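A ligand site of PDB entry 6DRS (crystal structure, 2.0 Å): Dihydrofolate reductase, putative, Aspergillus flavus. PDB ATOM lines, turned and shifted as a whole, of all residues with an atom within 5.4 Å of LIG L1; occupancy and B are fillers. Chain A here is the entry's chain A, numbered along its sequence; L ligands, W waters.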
ATOM      1  N   ILE A  10      -0.668 -13.838 -16.750  1.00  0.00           N
ATOM      2  CA  ILE A  10      -1.516 -13.094 -15.835  1.00  0.00           C
ATOM      3  C   ILE A  10      -2.092 -11.897 -16.588  1.00  0.00           C
ATOM      4  O   ILE A  10      -1.353 -11.173 -17.307  1.00  0.00           O
ATOM      5  CB  ILE A  10      -0.742 -12.666 -14.574  1.00  0.00           C
ATOM      6  CG1 ILE A  10      -1.667 -11.973 -13.582  1.00  0.00           C
ATOM      7  CG2 ILE A  10       0.488 -11.838 -14.920  1.00  0.00           C
ATOM      8  CD1 ILE A  10      -0.995 -11.549 -12.310  1.00  0.00           C
ATOM      9  N   VAL A  11      -3.391 -11.693 -16.391  1.00  0.00           N
ATOM     10  CA  VAL A  11      -4.168 -10.755 -17.238  1.00  0.00           C
ATOM     11  C   VAL A  11      -5.379 -10.275 -16.443  1.00  0.00           C
ATOM     12  O   VAL A  11      -5.886 -11.009 -15.583  1.00  0.00           O
ATOM     13  CB  VAL A  11      -4.614 -11.464 -18.532  1.00  0.00           C
ATOM     14  CG1 VAL A  11      -5.676 -12.520 -18.266  1.00  0.00           C
ATOM     15  CG2 VAL A  11      -5.088 -10.493 -19.619  1.00  0.00           C
ATOM     16  N   ALA A  12      -5.822  -9.035 -16.710  1.00  0.00           N
ATOM     17  CA  ALA A  12      -7.156  -8.588 -16.291  1.00  0.00           C
ATOM     18  C   ALA A  12      -8.055  -8.506 -17.551  1.00  0.00           C
ATOM     19  O   ALA A  12      -7.619  -8.000 -18.592  1.00  0.00           O
ATOM     20  CB  ALA A  12      -7.077  -7.273 -15.538  1.00  0.00           C
ATOM     21  N   LEU A  32      -4.930   0.479 -20.614  1.00  0.00           N
ATOM     22  CA  LEU A  32      -6.013  -0.412 -20.140  1.00  0.00           C
ATOM     23  C   LEU A  32      -7.368   0.214 -20.478  1.00  0.00           C
ATOM     24  O   LEU A  32      -7.449   1.406 -20.718  1.00  0.00           O
ATOM     25  CB  LEU A  32      -5.909  -0.658 -18.626  1.00  0.00           C
ATOM     26  CG  LEU A  32      -4.612  -1.311 -18.145  1.00  0.00           C
ATOM     27  CD1 LEU A  32      -4.609  -1.457 -16.633  1.00  0.00           C
ATOM     28  CD2 LEU A  32      -4.387  -2.666 -18.825  1.00  0.00           C
ATOM     29  N   ASP A  40      -6.530  -4.377  -8.354  1.00  0.00           N
ATOM     30  CA  ASP A  40      -5.911  -5.210  -9.401  1.00  0.00           C
ATOM     31  C   ASP A  40      -4.404  -4.912  -9.534  1.00  0.00           C
ATOM     32  O   ASP A  40      -3.614  -5.843  -9.677  1.00  0.00           O
ATOM     33  CB  ASP A  40      -6.613  -5.098 -10.752  1.00  0.00           C
ATOM     34  CG  ASP A  40      -5.893  -5.937 -11.789  1.00  0.00           C
ATOM     35  OD1 ASP A  40      -5.810  -7.173 -11.610  1.00  0.00           O
ATOM     36  OD2 ASP A  40      -5.348  -5.354 -12.753  1.00  0.00           O
ATOM     37  N   MET A  41      -4.043  -3.633  -9.500  1.00  0.00           N
ATOM     38  CA  MET A  41      -2.676  -3.128  -9.577  1.00  0.00           C
ATOM     39  C   MET A  41      -1.810  -3.720  -8.460  1.00  0.00           C
ATOM     40  O   MET A  41      -0.687  -4.162  -8.712  1.00  0.00           O
ATOM     41  CB  MET A  41      -2.644  -1.618  -9.348  1.00  0.00           C
ATOM     42  CG  MET A  41      -3.232  -0.828 -10.469  1.00  0.00           C
ATOM     43  SD  MET A  41      -2.301  -1.059 -11.988  1.00  0.00           S
ATOM     44  CE  MET A  41      -2.935   0.372 -12.882  1.00  0.00           C
ATOM     45  N   PHE A  43      -2.462  -6.308  -6.597  1.00  0.00           N
ATOM     46  CA  PHE A  43      -2.472  -7.730  -6.758  1.00  0.00           C
ATOM     47  C   PHE A  43      -1.449  -8.124  -7.827  1.00  0.00           C
ATOM     48  O   PHE A  43      -0.665  -9.066  -7.632  1.00  0.00           O
ATOM     49  CB  PHE A  43      -3.886  -8.265  -7.081  1.00  0.00           C
ATOM     50  CG  PHE A  43      -3.919  -9.725  -7.472  1.00  0.00           C
ATOM     51  CD1 PHE A  43      -4.016 -10.737  -6.512  1.00  0.00           C
ATOM     52  CD2 PHE A  43      -3.888 -10.117  -8.811  1.00  0.00           C
ATOM     53  CE1 PHE A  43      -4.088 -12.068  -6.876  1.00  0.00           C
ATOM     54  CE2 PHE A  43      -3.940 -11.456  -9.179  1.00  0.00           C
ATOM     55  CZ  PHE A  43      -4.029 -12.428  -8.213  1.00  0.00           C
ATOM     56  N   PHE A  44      -1.461  -7.421  -8.941  1.00  0.00           N
ATOM     57  CA  PHE A  44      -0.521  -7.713 -10.023  1.00  0.00           C
ATOM     58  C   PHE A  44       0.906  -7.525  -9.516  1.00  0.00           C
ATOM     59  O   PHE A  44       1.774  -8.312  -9.850  1.00  0.00           O
ATOM     60  CB  PHE A  44      -0.786  -6.833 -11.249  1.00  0.00           C
ATOM     61  CG  PHE A  44       0.304  -6.909 -12.301  1.00  0.00           C
ATOM     62  CD1 PHE A  44       0.297  -7.911 -13.266  1.00  0.00           C
ATOM     63  CD2 PHE A  44       1.333  -5.965 -12.328  1.00  0.00           C
ATOM     64  CE1 PHE A  44       1.294  -7.978 -14.240  1.00  0.00           C
ATOM     65  CE2 PHE A  44       2.332  -6.042 -13.293  1.00  0.00           C
ATOM     66  CZ  PHE A  44       2.317  -7.049 -14.238  1.00  0.00           C
ATOM     67  N   ALA A  45       1.116  -6.452  -8.745  1.00  0.00           N
ATOM     68  CA  ALA A  45       2.446  -6.079  -8.280  1.00  0.00           C
ATOM     69  C   ALA A  45       2.961  -7.154  -7.309  1.00  0.00           C
ATOM     70  O   ALA A  45       4.044  -7.705  -7.524  1.00  0.00           O
ATOM     71  CB  ALA A  45       2.428  -4.695  -7.669  1.00  0.00           C
ATOM     72  N   THR A  48       3.528 -10.637  -9.083  1.00  0.00           N
ATOM     73  CA  THR A  48       4.612 -10.779 -10.081  1.00  0.00           C
ATOM     74  C   THR A  48       5.974 -10.603  -9.396  1.00  0.00           C
ATOM     75  O   THR A  48       6.988 -11.051  -9.917  1.00  0.00           O
ATOM     76  CB  THR A  48       4.479  -9.766 -11.230  1.00  0.00           C
ATOM     77  OG1 THR A  48       4.386  -8.467 -10.625  1.00  0.00           O
ATOM     78  CG2 THR A  48       3.307 -10.047 -12.142  1.00  0.00           C
ATOM     79  N   THR A  66       3.195  -3.375 -24.558  1.00  0.00           N
ATOM     80  CA  THR A  66       2.863  -3.444 -23.135  1.00  0.00           C
ATOM     81  C   THR A  66       3.969  -2.764 -22.327  1.00  0.00           C
ATOM     82  O   THR A  66       3.700  -1.986 -21.405  1.00  0.00           O
ATOM     83  CB  THR A  66       2.628  -4.883 -22.670  1.00  0.00           C
ATOM     84  OG1 THR A  66       1.501  -5.398 -23.393  1.00  0.00           O
ATOM     85  CG2 THR A  66       2.356  -4.961 -21.187  1.00  0.00           C
ATOM     86  N   SER A  69       3.216   0.774 -22.583  1.00  0.00           N
ATOM     87  CA  SER A  69       1.974   1.136 -21.885  1.00  0.00           C
ATOM     88  C   SER A  69       2.239   1.549 -20.435  1.00  0.00           C
ATOM     89  O   SER A  69       1.419   2.267 -19.865  1.00  0.00           O
ATOM     90  CB  SER A  69       0.968   0.035 -21.923  1.00  0.00           C
ATOM     91  OG  SER A  69       1.308  -1.018 -21.061  1.00  0.00           O
ATOM     92  N   VAL A  70       3.346   1.076 -19.839  1.00  0.00           N
ATOM     93  CA  VAL A  70       3.702   1.520 -18.484  1.00  0.00           C
ATOM     94  C   VAL A  70       4.301   2.921 -18.592  1.00  0.00           C
ATOM     95  O   VAL A  70       5.160   3.129 -19.428  1.00  0.00           O
ATOM     96  CB  VAL A  70       4.728   0.583 -17.826  1.00  0.00           C
ATOM     97  CG1 VAL A  70       4.825   0.849 -16.342  1.00  0.00           C
ATOM     98  CG2 VAL A  70       4.415  -0.883 -18.091  1.00  0.00           C
ATOM     99  N   PRO A  71       3.879   3.848 -17.727  1.00  0.00           N
ATOM    100  CA  PRO A  71       4.444   5.213 -17.709  1.00  0.00           C
ATOM    101  C   PRO A  71       5.977   5.172 -17.563  1.00  0.00           C
ATOM    102  O   PRO A  71       6.487   4.294 -16.865  1.00  0.00           O
ATOM    103  CB  PRO A  71       3.820   5.904 -16.481  1.00  0.00           C
ATOM    104  CG  PRO A  71       2.597   5.063 -16.155  1.00  0.00           C
ATOM    105  CD  PRO A  71       2.948   3.664 -16.603  1.00  0.00           C
ATOM    106  N   LEU A  74       7.919   4.835 -14.190  1.00  0.00           N
ATOM    107  CA  LEU A  74       7.705   3.611 -13.443  1.00  0.00           C
ATOM    108  C   LEU A  74       8.414   2.453 -14.143  1.00  0.00           C
ATOM    109  O   LEU A  74       8.427   1.340 -13.646  1.00  0.00           O
ATOM    110  CB  LEU A  74       6.195   3.336 -13.326  1.00  0.00           C
ATOM    111  CG  LEU A  74       5.391   4.239 -12.393  1.00  0.00           C
ATOM    112  CD1 LEU A  74       4.215   3.469 -11.806  1.00  0.00           C
ATOM    113  CD2 LEU A  74       6.246   4.814 -11.259  1.00  0.00           C
ATOM    114  N   LEU A  77       9.757  -2.061 -14.591  1.00  0.00           N
ATOM    115  CA  LEU A  77       9.043  -2.195 -13.312  1.00  0.00           C
ATOM    116  C   LEU A  77       9.973  -2.821 -12.254  1.00  0.00           C
ATOM    117  O   LEU A  77      10.671  -3.822 -12.515  1.00  0.00           O
ATOM    118  CB  LEU A  77       7.813  -3.071 -13.581  1.00  0.00           C
ATOM    119  CG  LEU A  77       6.644  -2.364 -14.289  1.00  0.00           C
ATOM    120  CD1 LEU A  77       5.578  -3.369 -14.644  1.00  0.00           C
ATOM    121  CD2 LEU A  77       6.054  -1.279 -13.384  1.00  0.00           C
ATOM    122  N   ARG A  80      11.608  -6.842 -10.390  1.00  0.00           N
ATOM    123  CA  ARG A  80      11.435  -7.988 -11.257  1.00  0.00           C
ATOM    124  C   ARG A  80      12.426  -7.900 -12.429  1.00  0.00           C
ATOM    125  O   ARG A  80      13.014  -6.849 -12.680  1.00  0.00           O
ATOM    126  CB  ARG A  80       9.992  -8.018 -11.785  1.00  0.00           C
ATOM    127  CG  ARG A  80       8.975  -8.572 -10.793  1.00  0.00           C
ATOM    128  CD  ARG A  80       7.648  -7.869 -10.944  1.00  0.00           C
ATOM    129  NE  ARG A  80       7.706  -6.463 -10.524  1.00  0.00           N
ATOM    130  CZ  ARG A  80       6.681  -5.605 -10.536  1.00  0.00           C
ATOM    131  NH1 ARG A  80       5.464  -6.002 -10.873  1.00  0.00           N
ATOM    132  NH2 ARG A  80       6.887  -4.343 -10.196  1.00  0.00           N
ATOM    133  N   ILE A 156       3.077 -11.334 -19.106  1.00  0.00           N
ATOM    134  CA  ILE A 156       2.198 -10.243 -18.652  1.00  0.00           C
ATOM    135  C   ILE A 156       1.497  -9.528 -19.822  1.00  0.00           C
ATOM    136  O   ILE A 156       0.852  -8.488 -19.577  1.00  0.00           O
ATOM    137  CB  ILE A 156       2.930  -9.249 -17.718  1.00  0.00           C
ATOM    138  CG1 ILE A 156       3.960  -8.376 -18.451  1.00  0.00           C
ATOM    139  CG2 ILE A 156       3.565 -10.044 -16.574  1.00  0.00           C
ATOM    140  CD1 ILE A 156       4.262  -7.074 -17.767  1.00  0.00           C
ATOM    141  N   GLY A 157       1.550 -10.091 -21.038  1.00  0.00           N
ATOM    142  CA  GLY A 157       0.863  -9.440 -22.166  1.00  0.00           C
ATOM    143  C   GLY A 157       1.786  -8.753 -23.176  1.00  0.00           C
ATOM    144  O   GLY A 157       3.025  -8.795 -23.064  1.00  0.00           O
ATOM    145  N   TYR A 162       0.574 -13.016 -25.546  1.00  0.00           N
ATOM    146  CA  TYR A 162      -0.281 -14.082 -24.965  1.00  0.00           C
ATOM    147  C   TYR A 162      -0.569 -15.159 -26.021  1.00  0.00           C
ATOM    148  O   TYR A 162      -0.526 -16.367 -25.735  1.00  0.00           O
ATOM    149  CB  TYR A 162      -1.634 -13.555 -24.505  1.00  0.00           C
ATOM    150  CG  TYR A 162      -1.664 -12.703 -23.256  1.00  0.00           C
ATOM    151  CD1 TYR A 162      -0.976 -13.062 -22.112  1.00  0.00           C
ATOM    152  CD2 TYR A 162      -2.406 -11.539 -23.236  1.00  0.00           C
ATOM    153  CE1 TYR A 162      -1.026 -12.288 -20.968  1.00  0.00           C
ATOM    154  CE2 TYR A 162      -2.449 -10.732 -22.108  1.00  0.00           C
ATOM    155  CZ  TYR A 162      -1.779 -11.123 -20.958  1.00  0.00           C
ATOM    156  OH  TYR A 162      -1.830 -10.306 -19.874  1.00  0.00           O
ATOM    157  N   THR A 179      -7.902 -11.655 -13.642  1.00  0.00           N
ATOM    158  CA  THR A 179      -8.791 -10.804 -12.899  1.00  0.00           C
ATOM    159  C   THR A 179      -9.967 -10.425 -13.808  1.00  0.00           C
ATOM    160  O   THR A 179      -9.755  -9.794 -14.866  1.00  0.00           O
ATOM    161  CB  THR A 179      -8.102  -9.519 -12.417  1.00  0.00           C
ATOM    162  OG1 THR A 179      -6.912  -9.838 -11.696  1.00  0.00           O
ATOM    163  CG2 THR A 179      -9.047  -8.673 -11.575  1.00  0.00           C
HETATM  164  C1  LIG L   1      -1.198  -3.606 -15.271  1.00  0.00           C
HETATM  165  C2  LIG L   1      -2.133  -4.321 -14.504  1.00  0.00           C
HETATM  166  C3  LIG L   1      -2.307  -5.697 -14.716  1.00  0.00           C
HETATM  167  C4  LIG L   1      -1.575  -6.378 -15.719  1.00  0.00           C
HETATM  168  C5  LIG L   1      -0.624  -5.623 -16.457  1.00  0.00           C
HETATM  169  C6  LIG L   1      -0.484  -4.284 -16.241  1.00  0.00           C
HETATM  170  C7  LIG L   1      -1.767  -7.732 -15.886  1.00  0.00           C
HETATM  171  O1  LIG L   1      -1.006  -2.275 -15.074  1.00  0.00           O
HETATM  172  C8  LIG L   1      -3.363  -7.747 -14.178  1.00  0.00           C
HETATM  173  C9  LIG L   1       0.067  -1.737 -14.383  1.00  0.00           C
HETATM  174  C10 LIG L   1       0.386  -0.383 -14.591  1.00  0.00           C
HETATM  175  C11 LIG L   1       1.476   0.188 -13.907  1.00  0.00           C
HETATM  176  C12 LIG L   1       2.237  -0.606 -13.015  1.00  0.00           C
HETATM  177  C13 LIG L   1       1.939  -1.962 -12.789  1.00  0.00           C
HETATM  178  N1  LIG L   1      -2.665  -8.393 -15.125  1.00  0.00           N
HETATM  179  N2  LIG L   1      -3.214  -6.423 -13.995  1.00  0.00           N
HETATM  180  N3  LIG L   1      -0.974  -8.449 -16.876  1.00  0.00           N
HETATM  181  N4  LIG L   1      -4.340  -8.430 -13.335  1.00  0.00           N
HETATM  182  C14 LIG L   1       0.854  -2.516 -13.488  1.00  0.00           C
HETATM  183  C15 LIG L   1       2.682  -2.698 -11.948  1.00  0.00           C
HETATM  184  N5  LIG L   1       3.389  -3.355 -11.233  1.00  0.00           N
HETATM  185  C16 LIG L   1       0.520  -3.707 -17.137  1.00  0.00           C
HETATM  186  C17 LIG L   1       0.779  -4.892 -18.074  1.00  0.00           C
HETATM  187  O2  LIG L   1       0.206  -6.060 -17.454  1.00  0.00           O
HETATM  188  C18 LIG L   1       1.816  -3.565 -16.367  1.00  0.00           C
HETATM  189  P1  LG2 L   2       1.806  -6.558 -27.198  1.00  0.00           P
HETATM  190  O1  LG2 L   2       1.998  -6.000 -25.812  1.00  0.00           O
HETATM  191  O2  LG2 L   2       1.538  -7.960 -27.589  1.00  0.00           O
HETATM  192  O3  LG2 L   2       3.058  -6.040 -28.100  1.00  0.00           O
HETATM  193  C1  LG2 L   2       3.107  -6.118 -29.530  1.00  0.00           C
HETATM  194  C2  LG2 L   2       4.559  -5.877 -29.891  1.00  0.00           C
HETATM  195  O4  LG2 L   2       5.355  -6.939 -29.377  1.00  0.00           O
HETATM  196  C3  LG2 L   2       4.843  -5.894 -31.387  1.00  0.00           C
HETATM  197  O5  LG2 L   2       4.607  -4.595 -31.962  1.00  0.00           O
HETATM  198  C4  LG2 L   2       6.315  -6.274 -31.421  1.00  0.00           C
HETATM  199  O6  LG2 L   2       7.108  -5.184 -30.973  1.00  0.00           O
HETATM  200  C5  LG2 L   2       6.430  -7.261 -30.270  1.00  0.00           C
HETATM  201  N1  LG2 L   2       6.217  -8.621 -30.734  1.00  0.00           N
HETATM  202  C6  LG2 L   2       4.985  -9.174 -30.724  1.00  0.00           C
HETATM  203  N2  LG2 L   2       5.056 -10.436 -31.199  1.00  0.00           N
HETATM  204  C7  LG2 L   2       6.339 -10.702 -31.516  1.00  0.00           C
HETATM  205  C8  LG2 L   2       7.075 -11.868 -32.061  1.00  0.00           C
HETATM  206  N3  LG2 L   2       6.372 -12.977 -32.321  1.00  0.00           N
HETATM  207  N4  LG2 L   2       8.408 -11.797 -32.271  1.00  0.00           N
HETATM  208  C9  LG2 L   2       9.055 -10.661 -31.965  1.00  0.00           C
HETATM  209  N5  LG2 L   2       8.441  -9.553 -31.461  1.00  0.00           N
HETATM  210  C10 LG2 L   2       7.109  -9.494 -31.216  1.00  0.00           C
HETATM  211  O7  LG2 L   2       0.718  -5.545 -27.885  1.00  0.00           O
HETATM  212  P2  LG2 L   2      -0.898  -5.697 -28.017  1.00  0.00           P
HETATM  213  O8  LG2 L   2      -1.299  -7.083 -28.302  1.00  0.00           O
HETATM  214  O9  LG2 L   2      -1.241  -4.579 -28.971  1.00  0.00           O
HETATM  215  O10 LG2 L   2      -1.390  -5.284 -26.554  1.00  0.00           O
HETATM  216  C11 LG2 L   2      -1.088  -4.018 -26.019  1.00  0.00           C
HETATM  217  C12 LG2 L   2      -2.406  -3.611 -25.401  1.00  0.00           C
HETATM  218  O11 LG2 L   2      -2.819  -4.639 -24.506  1.00  0.00           O
HETATM  219  C13 LG2 L   2      -2.377  -2.311 -24.611  1.00  0.00           C
HETATM  220  O12 LG2 L   2      -3.663  -1.680 -24.809  1.00  0.00           O
HETATM  221  C14 LG2 L   2      -2.230  -2.805 -23.195  1.00  0.00           C
HETATM  222  O13 LG2 L   2      -2.741  -1.859 -22.289  1.00  0.00           O
HETATM  223  C15 LG2 L   2      -3.038  -4.087 -23.202  1.00  0.00           C
HETATM  224  N6  LG2 L   2      -2.619  -5.017 -22.134  1.00  0.00           N
HETATM  225  C16 LG2 L   2      -3.539  -5.358 -21.205  1.00  0.00           C
HETATM  226  C17 LG2 L   2      -3.221  -6.235 -20.143  1.00  0.00           C
HETATM  227  C18 LG2 L   2      -4.298  -6.605 -19.116  1.00  0.00           C
HETATM  228  O14 LG2 L   2      -4.061  -7.452 -18.242  1.00  0.00           O
HETATM  229  N7  LG2 L   2      -5.490  -5.991 -19.196  1.00  0.00           N
HETATM  230  C19 LG2 L   2      -1.909  -6.711 -20.039  1.00  0.00           C
HETATM  231  C20 LG2 L   2      -0.980  -6.326 -21.020  1.00  0.00           C
HETATM  232  C21 LG2 L   2      -1.351  -5.471 -22.053  1.00  0.00           C
HETATM  233  P3  LG2 L   2       7.822  -4.176 -32.011  1.00  0.00           P
HETATM  234  O15 LG2 L   2       6.685  -3.413 -32.696  1.00  0.00           O
HETATM  235  O16 LG2 L   2       8.542  -3.217 -31.099  1.00  0.00           O
HETATM  236  O17 LG2 L   2       8.509  -5.188 -32.869  1.00  0.00           O
HETATM  237  O   HOH W   1      -4.721 -11.417 -12.513  1.00  0.00           O
HETATM  238  O   HOH W   2       4.959  -2.162  -9.271  1.00  0.00           O
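The side-chain hydroxyl (OG1) of Thr 66 is in hydrogen-bond range of an oxygen (O1) of LG2 L2 (2.5 Å). The backbone NH (N) of Ala 12 is in hydrogen-bond range of an oxygen (O14) of LG2 L2, at 2.8 Å. The backbone carbonyl oxygen of Ile 156 sits at hydrogen-bond distance from a nitrogen (N3) of LIG L1 (3.3 Å). A nitrogen (N4) of LIG L1 lies within hydrogen-bond range of the side-chain carboxylate (OD1) of Asp 40 (2.6 Å). N5 of LIG L1 sits at hydrogen-bond distance from NH1 of Arg 80, 3.4 Å away. The backbone NH (N) of Thr 66 lies within hydrogen-bond range of an oxygen (O1) of LG2 L2 (3.1 Å). O of Ala 12 sits at hydrogen-bond distance from N7 of LG2 L2, at 3.0 Å. N3 of LIG L1 sits at hydrogen-bond distance from O of Ile 10, 2.8 Å away. A nitrogen (N4) of LIG L1 lies within hydrogen-bond range of the side-chain hydroxyl (OG1) of Thr 179, 3.4 Å away.
Water W2 lies within hydrogen-bond range of N5 of LIG L1 and NH2 of Arg 80. Water W1 lies within hydrogen-bond range of the side-chain hydroxyl (OG1) of Thr 179, a nitrogen (N4) of LIG L1 and the backbone carbonyl oxygen (O) of Val 11.
The side-chain sulfur (SD) of Met 41 sits close to an oxygen (O1) of LIG L1. Val 11 touches LIG L1. N of Ala 12 touches N1 of LIG L1, at 3.6 Å. Phe 44 touches LIG L1. Ala 45 touches LIG L1 (CB to N5, 3.9 Å). Thr 66 touches LIG L1. Leu 77 touches LIG L1 (CD2 to C12, 3.9 Å). Tyr 162 touches LIG L1. Hydrophobic or aromatic side chains within 4 Å of LIG L1: Ala 12, Met 41, Phe 44, Ala 45 and Leu 77. 13 residues have an atom within 4 Å of LIG L1: Ile 10, Val 11, Ala 12, Asp 40, Met 41, Phe 44, Ala 45, Thr 66, Leu 77, Arg 80, Ile 156, Tyr 162 and Thr 179.
The side-chain hydroxyl (OG1) of Thr 179 is in hydrogen-bond range of the side-chain carboxylate (OD1) of Asp 40. OG1 of Thr 48 sits at hydrogen-bond distance from O of Phe 44. The backbone carbonyl oxygen of Thr 66 lies within hydrogen-bond range of the side-chain hydroxyl of Ser 69, at 2.6 Å. O of Ile 156 sits at hydrogen-bond distance from OH of Tyr 162 (3.3 Å). The backbone carbonyl oxygen (O) of Ile 10 is in hydrogen-bond range of the side-chain hydroxyl (OH) of Tyr 162 (2.8 Å). The guanidinium group of Arg 80 sits at hydrogen-bond distance from the side-chain hydroxyl of Thr 48. The backbone carbonyl oxygen (O) of Ala 45 is in hydrogen-bond range of the side-chain hydroxyl (OG1) of Thr 48 (3.2 Å). The backbone NH of Thr 179 lies within hydrogen-bond range of the backbone carbonyl oxygen of Val 11, at 2.9 Å.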
